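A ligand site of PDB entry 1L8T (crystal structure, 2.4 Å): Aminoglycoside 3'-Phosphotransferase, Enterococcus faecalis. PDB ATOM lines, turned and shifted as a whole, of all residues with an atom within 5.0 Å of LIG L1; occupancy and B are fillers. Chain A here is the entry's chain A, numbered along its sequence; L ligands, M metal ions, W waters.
OE1 of Glu 156 lies within salt-bridge range of N1 of LIG L1, at 3.0 Å.
The backbone NH (N) of Met 25 sits at hydrogen-bond distance from an oxygen (O2) of LG2 L2 (3.5 Å).
A nitrogen (N3) of LIG L1 sits at hydrogen-bond distance from the backbone carbonyl oxygen of Asn 157, 2.8 Å away.
A nitrogen (N4) of LIG L1 is in salt-bridge range of the side-chain carboxylate (OE2) of Glu 229, 3.0 Å away.
The side-chain carboxylate (OE2) of Glu 261 lies within salt-bridge range of a nitrogen (N3) of LIG L1, 2.9 Å away.
A nitrogen (N2) of LIG L1 lies within salt-bridge range of the side-chain carboxylate (OD2) of Asp 260.
OXT of Phe 263 lies within salt-bridge range of N1 of LIG L1.
The backbone carbonyl oxygen (O) of Asp 260 sits at hydrogen-bond distance from a nitrogen (N2) of LIG L1, 3.0 Å away.
The side-chain carboxylate (OE2) of Glu 159 is in salt-bridge range of a nitrogen (N3) of LIG L1, at 3.0 Å.
An oxygen (O2) of LG2 L2 sits close to the backbone NH (N) of Ser 26, at 3.2 Å.
An oxygen (O3) of LIG L1 sits at hydrogen-bond distance from the side-chain carboxylate (OD2) of Asp 189.
O2 of LG2 L2 is in hydrogen-bond range of OG of Ser 26, 2.6 Å away.
The guanidinium group of Arg 225 sits at hydrogen-bond distance from an oxygen (O11) of LIG L1 (3.5 Å).
O of Asp 189 is in hydrogen-bond range of ND2 of Asn 194 (2.8 Å).
The side-chain carboxylate (OD2) of Asp 260 is in salt-bridge range of the guanidinium group (NH2) of Arg 225 (2.7 Å).
N of Glu 159 is in hydrogen-bond range of OE1 of Glu 261, at 2.7 Å.
Met 25 touches LIG L1.
Trp 158 touches LIG L1.
Ser 226 touches LIG L1.
Hydrophobic or aromatic side chains that line LIG L1: Met 25.
Within 4 Å of LIG L1: Met 25, Glu 156, Asn 157, Trp 158, Glu 159, Asp 189, Arg 225, Ser 226, Glu 229, Asp 260, Glu 261 and Phe 263.
The nearest printed residue that does not touch LIG L1 is Ser 26 (4.03 Å).
Water W6 lies within hydrogen-bond range of O10 of LIG L1 (2.5 Å), OG of Ser 226 (2.6 Å) and NE of Arg 225 (3.0 Å).
Water W4 lies within hydrogen-bond range of an oxygen (O3) of LIG L1 (2.5 Å) and an oxygen (O2) of LG2 L2 (3.4 Å).
Water W3 lies within hydrogen-bond range of an oxygen (O3) of LIG L1, the side-chain carboxylate (OD2) of Asp 189 and the side-chain amide nitrogen (ND2) of Asn 194.
Water W8 lies within hydrogen-bond range of N4 of LIG L1 (2.7 Å), OE1 of Glu 159 (2.8 Å) and O of Arg 225 (3.0 Å).
Water W5 bridges the guanidinium group of Arg 225 (2.6 Å) and the side-chain carboxylate of Glu 261 (2.8 Å).
Water W1 lies within hydrogen-bond range of the side-chain carboxylate of Asp 189 (2.5 Å) and an oxygen (O3) of LIG L1 (3.5 Å).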
ATOM      1  N   MET A  25     -14.332  21.528 -11.008  1.00  0.00           N
ATOM      2  CA  MET A  25     -13.225  21.292 -10.102  1.00  0.00           C
ATOM      3  C   MET A  25     -12.716  19.865 -10.213  1.00  0.00           C
ATOM      4  O   MET A  25     -11.775  19.471  -9.516  1.00  0.00           O
ATOM      5  CB  MET A  25     -13.662  21.567  -8.662  1.00  0.00           C
ATOM      6  CG  MET A  25     -13.923  23.022  -8.364  1.00  0.00           C
ATOM      7  SD  MET A  25     -15.068  23.228  -6.993  1.00  0.00           S
ATOM      8  CE  MET A  25     -14.038  22.676  -5.579  1.00  0.00           C
ATOM      9  N   SER A  26     -13.334  19.089 -11.080  1.00  0.00           N
ATOM     10  CA  SER A  26     -12.912  17.706 -11.239  1.00  0.00           C
ATOM     11  C   SER A  26     -11.640  17.645 -12.069  1.00  0.00           C
ATOM     12  O   SER A  26     -11.119  18.672 -12.502  1.00  0.00           O
ATOM     13  CB  SER A  26     -14.004  16.895 -11.956  1.00  0.00           C
ATOM     14  OG  SER A  26     -14.066  17.220 -13.321  1.00  0.00           O
ATOM     15  N   TYR A  54     -14.970   8.971 -12.293  1.00  0.00           N
ATOM     16  CA  TYR A  54     -14.587  10.222 -12.927  1.00  0.00           C
ATOM     17  C   TYR A  54     -14.543  10.051 -14.443  1.00  0.00           C
ATOM     18  O   TYR A  54     -14.729  11.007 -15.200  1.00  0.00           O
ATOM     19  CB  TYR A  54     -13.207  10.666 -12.461  1.00  0.00           C
ATOM     20  CG  TYR A  54     -13.099  11.083 -11.019  1.00  0.00           C
ATOM     21  CD1 TYR A  54     -12.487  10.259 -10.073  1.00  0.00           C
ATOM     22  CD2 TYR A  54     -13.591  12.315 -10.595  1.00  0.00           C
ATOM     23  CE1 TYR A  54     -12.361  10.665  -8.741  1.00  0.00           C
ATOM     24  CE2 TYR A  54     -13.467  12.724  -9.280  1.00  0.00           C
ATOM     25  CZ  TYR A  54     -12.857  11.905  -8.351  1.00  0.00           C
ATOM     26  OH  TYR A  54     -12.745  12.339  -7.059  1.00  0.00           O
ATOM     27  N   GLU A 156      -7.960  20.492  -0.540  1.00  0.00           N
ATOM     28  CA  GLU A 156      -9.359  20.424  -0.941  1.00  0.00           C
ATOM     29  C   GLU A 156     -10.172  21.348  -0.012  1.00  0.00           C
ATOM     30  O   GLU A 156      -9.699  21.737   1.056  1.00  0.00           O
ATOM     31  CB  GLU A 156      -9.868  18.984  -0.822  1.00  0.00           C
ATOM     32  CG  GLU A 156     -11.365  18.756  -1.102  1.00  0.00           C
ATOM     33  CD  GLU A 156     -11.703  18.698  -2.591  1.00  0.00           C
ATOM     34  OE1 GLU A 156     -10.896  18.144  -3.369  1.00  0.00           O
ATOM     35  OE2 GLU A 156     -12.793  19.182  -2.977  1.00  0.00           O
ATOM     36  N   ASN A 157     -11.388  21.709  -0.421  1.00  0.00           N
ATOM     37  CA  ASN A 157     -12.257  22.586   0.384  1.00  0.00           C
ATOM     38  C   ASN A 157     -13.117  21.721   1.290  1.00  0.00           C
ATOM     39  O   ASN A 157     -14.265  21.396   0.966  1.00  0.00           O
ATOM     40  CB  ASN A 157     -13.146  23.445  -0.525  1.00  0.00           C
ATOM     41  CG  ASN A 157     -14.174  24.275   0.254  1.00  0.00           C
ATOM     42  OD1 ASN A 157     -15.218  24.643  -0.279  1.00  0.00           O
ATOM     43  ND2 ASN A 157     -13.866  24.589   1.510  1.00  0.00           N
ATOM     44  N   TRP A 158     -12.559  21.355   2.439  1.00  0.00           N
ATOM     45  CA  TRP A 158     -13.245  20.502   3.403  1.00  0.00           C
ATOM     46  C   TRP A 158     -14.287  21.215   4.258  1.00  0.00           C
ATOM     47  O   TRP A 158     -14.228  22.419   4.446  1.00  0.00           O
ATOM     48  CB  TRP A 158     -12.215  19.837   4.324  1.00  0.00           C
ATOM     49  CG  TRP A 158     -11.236  18.978   3.608  1.00  0.00           C
ATOM     50  CD1 TRP A 158     -11.509  17.863   2.848  1.00  0.00           C
ATOM     51  CD2 TRP A 158      -9.823  19.142   3.574  1.00  0.00           C
ATOM     52  NE1 TRP A 158     -10.342  17.330   2.340  1.00  0.00           N
ATOM     53  CE2 TRP A 158      -9.292  18.094   2.772  1.00  0.00           C
ATOM     54  CE3 TRP A 158      -8.942  20.066   4.142  1.00  0.00           C
ATOM     55  CZ2 TRP A 158      -7.923  17.966   2.524  1.00  0.00           C
ATOM     56  CZ3 TRP A 158      -7.579  19.932   3.900  1.00  0.00           C
ATOM     57  CH2 TRP A 158      -7.085  18.890   3.102  1.00  0.00           C
ATOM     58  N   GLU A 159     -15.242  20.422   4.766  1.00  0.00           N
ATOM     59  CA  GLU A 159     -16.282  20.937   5.638  1.00  0.00           C
ATOM     60  C   GLU A 159     -15.637  21.359   6.949  1.00  0.00           C
ATOM     61  O   GLU A 159     -14.715  20.701   7.436  1.00  0.00           O
ATOM     62  CB  GLU A 159     -17.332  19.853   5.914  1.00  0.00           C
ATOM     63  CG  GLU A 159     -18.068  19.311   4.704  1.00  0.00           C
ATOM     64  CD  GLU A 159     -18.843  20.380   3.967  1.00  0.00           C
ATOM     65  OE1 GLU A 159     -19.683  21.058   4.603  1.00  0.00           O
ATOM     66  OE2 GLU A 159     -18.621  20.540   2.750  1.00  0.00           O
ATOM     67  N   ASP A 189     -23.433  13.656  -7.535  1.00  0.00           N
ATOM     68  CA  ASP A 189     -22.866  14.960  -7.202  1.00  0.00           C
ATOM     69  C   ASP A 189     -23.917  16.022  -7.444  1.00  0.00           C
ATOM     70  O   ASP A 189     -23.787  16.892  -8.311  1.00  0.00           O
ATOM     71  CB  ASP A 189     -21.608  15.215  -8.034  1.00  0.00           C
ATOM     72  CG  ASP A 189     -20.898  16.496  -7.641  1.00  0.00           C
ATOM     73  OD1 ASP A 189     -21.107  17.006  -6.513  1.00  0.00           O
ATOM     74  OD2 ASP A 189     -20.123  17.003  -8.474  1.00  0.00           O
ATOM     75  N   ASN A 194     -24.418  21.381 -11.296  1.00  0.00           N
ATOM     76  CA  ASN A 194     -24.703  20.293 -12.216  1.00  0.00           C
ATOM     77  C   ASN A 194     -26.184  20.164 -12.571  1.00  0.00           C
ATOM     78  O   ASN A 194     -26.575  19.227 -13.272  1.00  0.00           O
ATOM     79  CB  ASN A 194     -24.203  18.967 -11.624  1.00  0.00           C
ATOM     80  CG  ASN A 194     -22.736  19.009 -11.233  1.00  0.00           C
ATOM     81  OD1 ASN A 194     -21.889  19.439 -12.017  1.00  0.00           O
ATOM     82  ND2 ASN A 194     -22.421  18.570 -10.026  1.00  0.00           N
ATOM     83  N   ASP A 207     -22.788  16.053 -15.428  1.00  0.00           N
ATOM     84  CA  ASP A 207     -21.817  15.498 -14.502  1.00  0.00           C
ATOM     85  C   ASP A 207     -22.411  14.172 -14.008  1.00  0.00           C
ATOM     86  O   ASP A 207     -22.917  14.102 -12.897  1.00  0.00           O
ATOM     87  CB  ASP A 207     -21.644  16.469 -13.325  1.00  0.00           C
ATOM     88  CG  ASP A 207     -20.204  16.577 -12.847  1.00  0.00           C
ATOM     89  OD1 ASP A 207     -19.418  15.612 -13.013  1.00  0.00           O
ATOM     90  OD2 ASP A 207     -19.872  17.624 -12.277  1.00  0.00           O
ATOM     91  N   ARG A 210     -20.641   9.697 -11.837  1.00  0.00           N
ATOM     92  CA  ARG A 210     -20.881   9.080 -10.534  1.00  0.00           C
ATOM     93  C   ARG A 210     -22.315   8.595 -10.347  1.00  0.00           C
ATOM     94  O   ARG A 210     -22.686   8.198  -9.240  1.00  0.00           O
ATOM     95  CB  ARG A 210     -20.546  10.086  -9.440  1.00  0.00           C
ATOM     96  CG  ARG A 210     -20.064   9.478  -8.147  1.00  0.00           C
ATOM     97  CD  ARG A 210     -19.668  10.570  -7.152  1.00  0.00           C
ATOM     98  NE  ARG A 210     -18.596  11.450  -7.634  1.00  0.00           N
ATOM     99  CZ  ARG A 210     -17.375  11.038  -7.989  1.00  0.00           C
ATOM    100  NH1 ARG A 210     -17.073   9.757  -7.927  1.00  0.00           N
ATOM    101  NH2 ARG A 210     -16.462  11.894  -8.409  1.00  0.00           N
ATOM    102  N   ARG A 225     -26.195  19.703   2.567  1.00  0.00           N
ATOM    103  CA  ARG A 225     -24.885  20.327   2.622  1.00  0.00           C
ATOM    104  C   ARG A 225     -24.886  21.678   1.916  1.00  0.00           C
ATOM    105  O   ARG A 225     -24.402  22.666   2.472  1.00  0.00           O
ATOM    106  CB  ARG A 225     -23.825  19.399   2.015  1.00  0.00           C
ATOM    107  CG  ARG A 225     -22.398  19.875   2.241  1.00  0.00           C
ATOM    108  CD  ARG A 225     -21.394  19.027   1.490  1.00  0.00           C
ATOM    109  NE  ARG A 225     -21.632  19.036   0.043  1.00  0.00           N
ATOM    110  CZ  ARG A 225     -20.906  18.364  -0.837  1.00  0.00           C
ATOM    111  NH1 ARG A 225     -21.202  18.424  -2.132  1.00  0.00           N
ATOM    112  NH2 ARG A 225     -19.883  17.628  -0.446  1.00  0.00           N
ATOM    113  N   SER A 226     -25.408  21.740   0.693  1.00  0.00           N
ATOM    114  CA  SER A 226     -25.468  22.996  -0.040  1.00  0.00           C
ATOM    115  C   SER A 226     -26.323  23.969   0.760  1.00  0.00           C
ATOM    116  O   SER A 226     -25.894  25.060   1.124  1.00  0.00           O
ATOM    117  CB  SER A 226     -26.112  22.826  -1.415  1.00  0.00           C
ATOM    118  OG  SER A 226     -25.351  21.992  -2.255  1.00  0.00           O
ATOM    119  N   GLU A 229     -24.957  25.730   3.749  1.00  0.00           N
ATOM    120  CA  GLU A 229     -23.894  26.695   3.500  1.00  0.00           C
ATOM    121  C   GLU A 229     -24.357  27.886   2.668  1.00  0.00           C
ATOM    122  O   GLU A 229     -23.946  29.013   2.916  1.00  0.00           O
ATOM    123  CB  GLU A 229     -22.685  26.063   2.802  1.00  0.00           C
ATOM    124  CG  GLU A 229     -21.506  27.034   2.734  1.00  0.00           C
ATOM    125  CD  GLU A 229     -20.551  26.783   1.576  1.00  0.00           C
ATOM    126  OE1 GLU A 229     -21.035  26.499   0.466  1.00  0.00           O
ATOM    127  OE2 GLU A 229     -19.316  26.883   1.785  1.00  0.00           O
ATOM    128  N   ASP A 230     -25.205  27.629   1.676  1.00  0.00           N
ATOM    129  CA  ASP A 230     -25.691  28.672   0.773  1.00  0.00           C
ATOM    130  C   ASP A 230     -26.883  29.502   1.281  1.00  0.00           C
ATOM    131  O   ASP A 230     -27.260  30.469   0.631  1.00  0.00           O
ATOM    132  CB  ASP A 230     -26.052  28.066  -0.589  1.00  0.00           C
ATOM    133  CG  ASP A 230     -24.854  27.421  -1.276  1.00  0.00           C
ATOM    134  OD1 ASP A 230     -25.046  26.714  -2.289  1.00  0.00           O
ATOM    135  OD2 ASP A 230     -23.715  27.615  -0.808  1.00  0.00           O
ATOM    136  N   ASP A 260     -17.987  12.214   0.625  1.00  0.00           N
ATOM    137  CA  ASP A 260     -17.628  13.040  -0.520  1.00  0.00           C
ATOM    138  C   ASP A 260     -16.359  13.841  -0.317  1.00  0.00           C
ATOM    139  O   ASP A 260     -15.761  14.340  -1.267  1.00  0.00           O
ATOM    140  CB  ASP A 260     -18.787  13.985  -0.855  1.00  0.00           C
ATOM    141  CG  ASP A 260     -18.609  14.671  -2.186  1.00  0.00           C
ATOM    142  OD1 ASP A 260     -18.384  13.961  -3.186  1.00  0.00           O
ATOM    143  OD2 ASP A 260     -18.698  15.923  -2.230  1.00  0.00           O
ATOM    144  N   GLU A 261     -15.950  13.959   0.936  1.00  0.00           N
ATOM    145  CA  GLU A 261     -14.784  14.733   1.300  1.00  0.00           C
ATOM    146  C   GLU A 261     -13.518  14.482   0.466  1.00  0.00           C
ATOM    147  O   GLU A 261     -12.908  15.428  -0.022  1.00  0.00           O
ATOM    148  CB  GLU A 261     -14.504  14.515   2.777  1.00  0.00           C
ATOM    149  CG  GLU A 261     -14.115  15.760   3.538  1.00  0.00           C
ATOM    150  CD  GLU A 261     -15.076  16.908   3.348  1.00  0.00           C
ATOM    151  OE1 GLU A 261     -15.067  17.819   4.200  1.00  0.00           O
ATOM    152  OE2 GLU A 261     -15.823  16.926   2.360  1.00  0.00           O
ATOM    153  N   PHE A 263     -13.327  13.024  -2.534  1.00  0.00           N
ATOM    154  CA  PHE A 263     -13.525  12.910  -3.987  1.00  0.00           C
ATOM    155  C   PHE A 263     -13.420  14.259  -4.708  1.00  0.00           C
ATOM    156  O   PHE A 263     -13.449  14.232  -5.955  1.00  0.00           O
ATOM    157  CB  PHE A 263     -14.874  12.258  -4.317  1.00  0.00           C
ATOM    158  CG  PHE A 263     -14.911  10.774  -4.074  1.00  0.00           C
ATOM    159  CD1 PHE A 263     -15.291  10.256  -2.832  1.00  0.00           C
ATOM    160  CD2 PHE A 263     -14.536   9.881  -5.085  1.00  0.00           C
ATOM    161  CE1 PHE A 263     -15.304   8.887  -2.597  1.00  0.00           C
ATOM    162  CE2 PHE A 263     -14.546   8.501  -4.840  1.00  0.00           C
ATOM    163  CZ  PHE A 263     -14.932   8.011  -3.610  1.00  0.00           C
ATOM    164  OXT PHE A 263     -13.318  15.301  -4.019  1.00  0.00           O
HETATM  165  C1  LIG L   1     -16.020  19.591  -5.364  1.00  0.00           C
HETATM  166  C2  LIG L   1     -16.989  19.687  -6.537  1.00  0.00           C
HETATM  167  C3  LIG L   1     -17.070  18.362  -7.252  1.00  0.00           C
HETATM  168  C4  LIG L   1     -15.681  17.950  -7.687  1.00  0.00           C
HETATM  169  C5  LIG L   1     -14.823  17.803  -6.451  1.00  0.00           C
HETATM  170  C6  LIG L   1     -13.409  17.382  -6.848  1.00  0.00           C
HETATM  171  C7  LIG L   1     -16.699  19.111  -0.215  1.00  0.00           C
HETATM  172  C8  LIG L   1     -16.902  20.377  -1.065  1.00  0.00           C
HETATM  173  C9  LIG L   1     -17.214  19.978  -2.528  1.00  0.00           C
HETATM  174  C10 LIG L   1     -16.133  19.058  -3.099  1.00  0.00           C
HETATM  175  C11 LIG L   1     -16.038  17.808  -2.220  1.00  0.00           C
HETATM  176  C12 LIG L   1     -15.621  18.205  -0.813  1.00  0.00           C
HETATM  177  C13 LIG L   1     -17.833  22.490  -0.665  1.00  0.00           C
HETATM  178  C14 LIG L   1     -18.216  23.244   0.618  1.00  0.00           C
HETATM  179  C15 LIG L   1     -19.695  23.089   0.921  1.00  0.00           C
HETATM  180  C16 LIG L   1     -20.517  23.471  -0.279  1.00  0.00           C
HETATM  181  C17 LIG L   1     -20.093  22.579  -1.448  1.00  0.00           C
HETATM  182  C18 LIG L   1     -20.913  22.897  -2.685  1.00  0.00           C
HETATM  183  N1  LIG L   1     -12.597  17.151  -5.650  1.00  0.00           N
HETATM  184  N2  LIG L   1     -15.033  16.878  -2.775  1.00  0.00           N
HETATM  185  N3  LIG L   1     -16.309  19.487   1.154  1.00  0.00           N
HETATM  186  N4  LIG L   1     -20.038  23.955   2.053  1.00  0.00           N
HETATM  187  O1  LIG L   1     -14.733  19.060  -5.768  1.00  0.00           O
HETATM  188  O2  LIG L   1     -18.291  20.014  -6.044  1.00  0.00           O
HETATM  189  O3  LIG L   1     -17.884  18.528  -8.393  1.00  0.00           O
HETATM  190  O4  LIG L   1     -15.776  16.689  -8.340  1.00  0.00           O
HETATM  191  O5  LIG L   1     -16.491  18.636  -4.410  1.00  0.00           O
HETATM  192  O6  LIG L   1     -17.278  21.148  -3.333  1.00  0.00           O
HETATM  193  O7  LIG L   1     -18.015  21.076  -0.526  1.00  0.00           O
HETATM  194  O8  LIG L   1     -18.708  22.835  -1.757  1.00  0.00           O
HETATM  195  O9  LIG L   1     -17.483  22.697   1.690  1.00  0.00           O
HETATM  196  O10 LIG L   1     -21.880  23.219   0.041  1.00  0.00           O
HETATM  197  O11 LIG L   1     -21.130  21.670  -3.380  1.00  0.00           O
HETATM  198  P1  LG2 L   2     -17.053  18.676 -13.377  1.00  0.00           P
HETATM  199  O1  LG2 L   2     -17.259  17.233 -13.242  1.00  0.00           O
HETATM  200  O2  LG2 L   2     -15.719  19.257 -13.268  1.00  0.00           O
HETATM  201  O3  LG2 L   2     -17.960  19.426 -12.299  1.00  0.00           O
HETATM  202  P2  LG2 L   2     -19.145  19.438 -15.184  1.00  0.00           P
HETATM  203  O4  LG2 L   2     -19.657  18.379 -16.097  1.00  0.00           O
HETATM  204  O5  LG2 L   2     -19.874  19.777 -13.949  1.00  0.00           O
HETATM  205  O6  LG2 L   2     -17.626  19.092 -14.816  1.00  0.00           O
HETATM  206  O7  LG2 L   2     -18.987  20.774 -16.037  1.00  0.00           O
HETATM  207  C1  LG2 L   2     -18.430  21.949 -15.440  1.00  0.00           C
HETATM  208  C2  LG2 L   2     -19.293  23.153 -15.780  1.00  0.00           C
HETATM  209  O8  LG2 L   2     -19.393  23.295 -17.199  1.00  0.00           O
HETATM  210  C3  LG2 L   2     -20.767  23.010 -15.339  1.00  0.00           C
HETATM  211  O9  LG2 L   2     -20.945  23.643 -14.063  1.00  0.00           O
HETATM  212  C4  LG2 L   2     -21.471  23.826 -16.421  1.00  0.00           C
HETATM  213  O10 LG2 L   2     -21.307  25.218 -16.136  1.00  0.00           O
HETATM  214  C5  LG2 L   2     -20.715  23.528 -17.690  1.00  0.00           C
HETATM  215  N1  LG2 L   2     -21.283  22.447 -18.520  1.00  0.00           N
HETATM  216  C6  LG2 L   2     -20.828  21.158 -18.722  1.00  0.00           C
HETATM  217  N2  LG2 L   2     -21.568  20.446 -19.535  1.00  0.00           N
HETATM  218  C7  LG2 L   2     -22.575  21.324 -19.891  1.00  0.00           C
HETATM  219  C8  LG2 L   2     -23.716  21.201 -20.747  1.00  0.00           C
HETATM  220  N3  LG2 L   2     -24.008  20.094 -21.422  1.00  0.00           N
HETATM  221  N4  LG2 L   2     -24.523  22.298 -20.877  1.00  0.00           N
HETATM  222  C9  LG2 L   2     -24.242  23.432 -20.202  1.00  0.00           C
HETATM  223  N5  LG2 L   2     -23.213  23.662 -19.385  1.00  0.00           N
HETATM  224  C10 LG2 L   2     -22.410  22.539 -19.272  1.00  0.00           C
HETATM  225 MG    MG M   1     -17.807  16.186 -11.685  1.00  0.00          MG
HETATM  226 MG    MG M   2     -20.042  19.591 -12.150  1.00  0.00          MG
HETATM  227  O   HOH W   1     -18.918  15.766 -10.273  1.00  0.00           O
HETATM  228  O   HOH W   2     -17.756  25.451   3.055  1.00  0.00           O
HETATM  229  O   HOH W   3     -19.433  19.285 -10.240  1.00  0.00           O
HETATM  230  O   HOH W   4     -17.103  17.672 -10.614  1.00  0.00           O
HETATM  231  O   HOH W   5     -18.466  16.730   1.489  1.00  0.00           O
HETATM  232  O   HOH W   6     -23.011  21.386  -1.188  1.00  0.00           O
HETATM  233  O   HOH W   7     -16.735  20.178  -9.966  1.00  0.00           O
HETATM  234  O   HOH W   8     -21.710  22.824   3.787  1.00  0.00           O
HETATM  235  O   HOH W   9     -19.542  17.632  -4.211  1.00  0.00           O
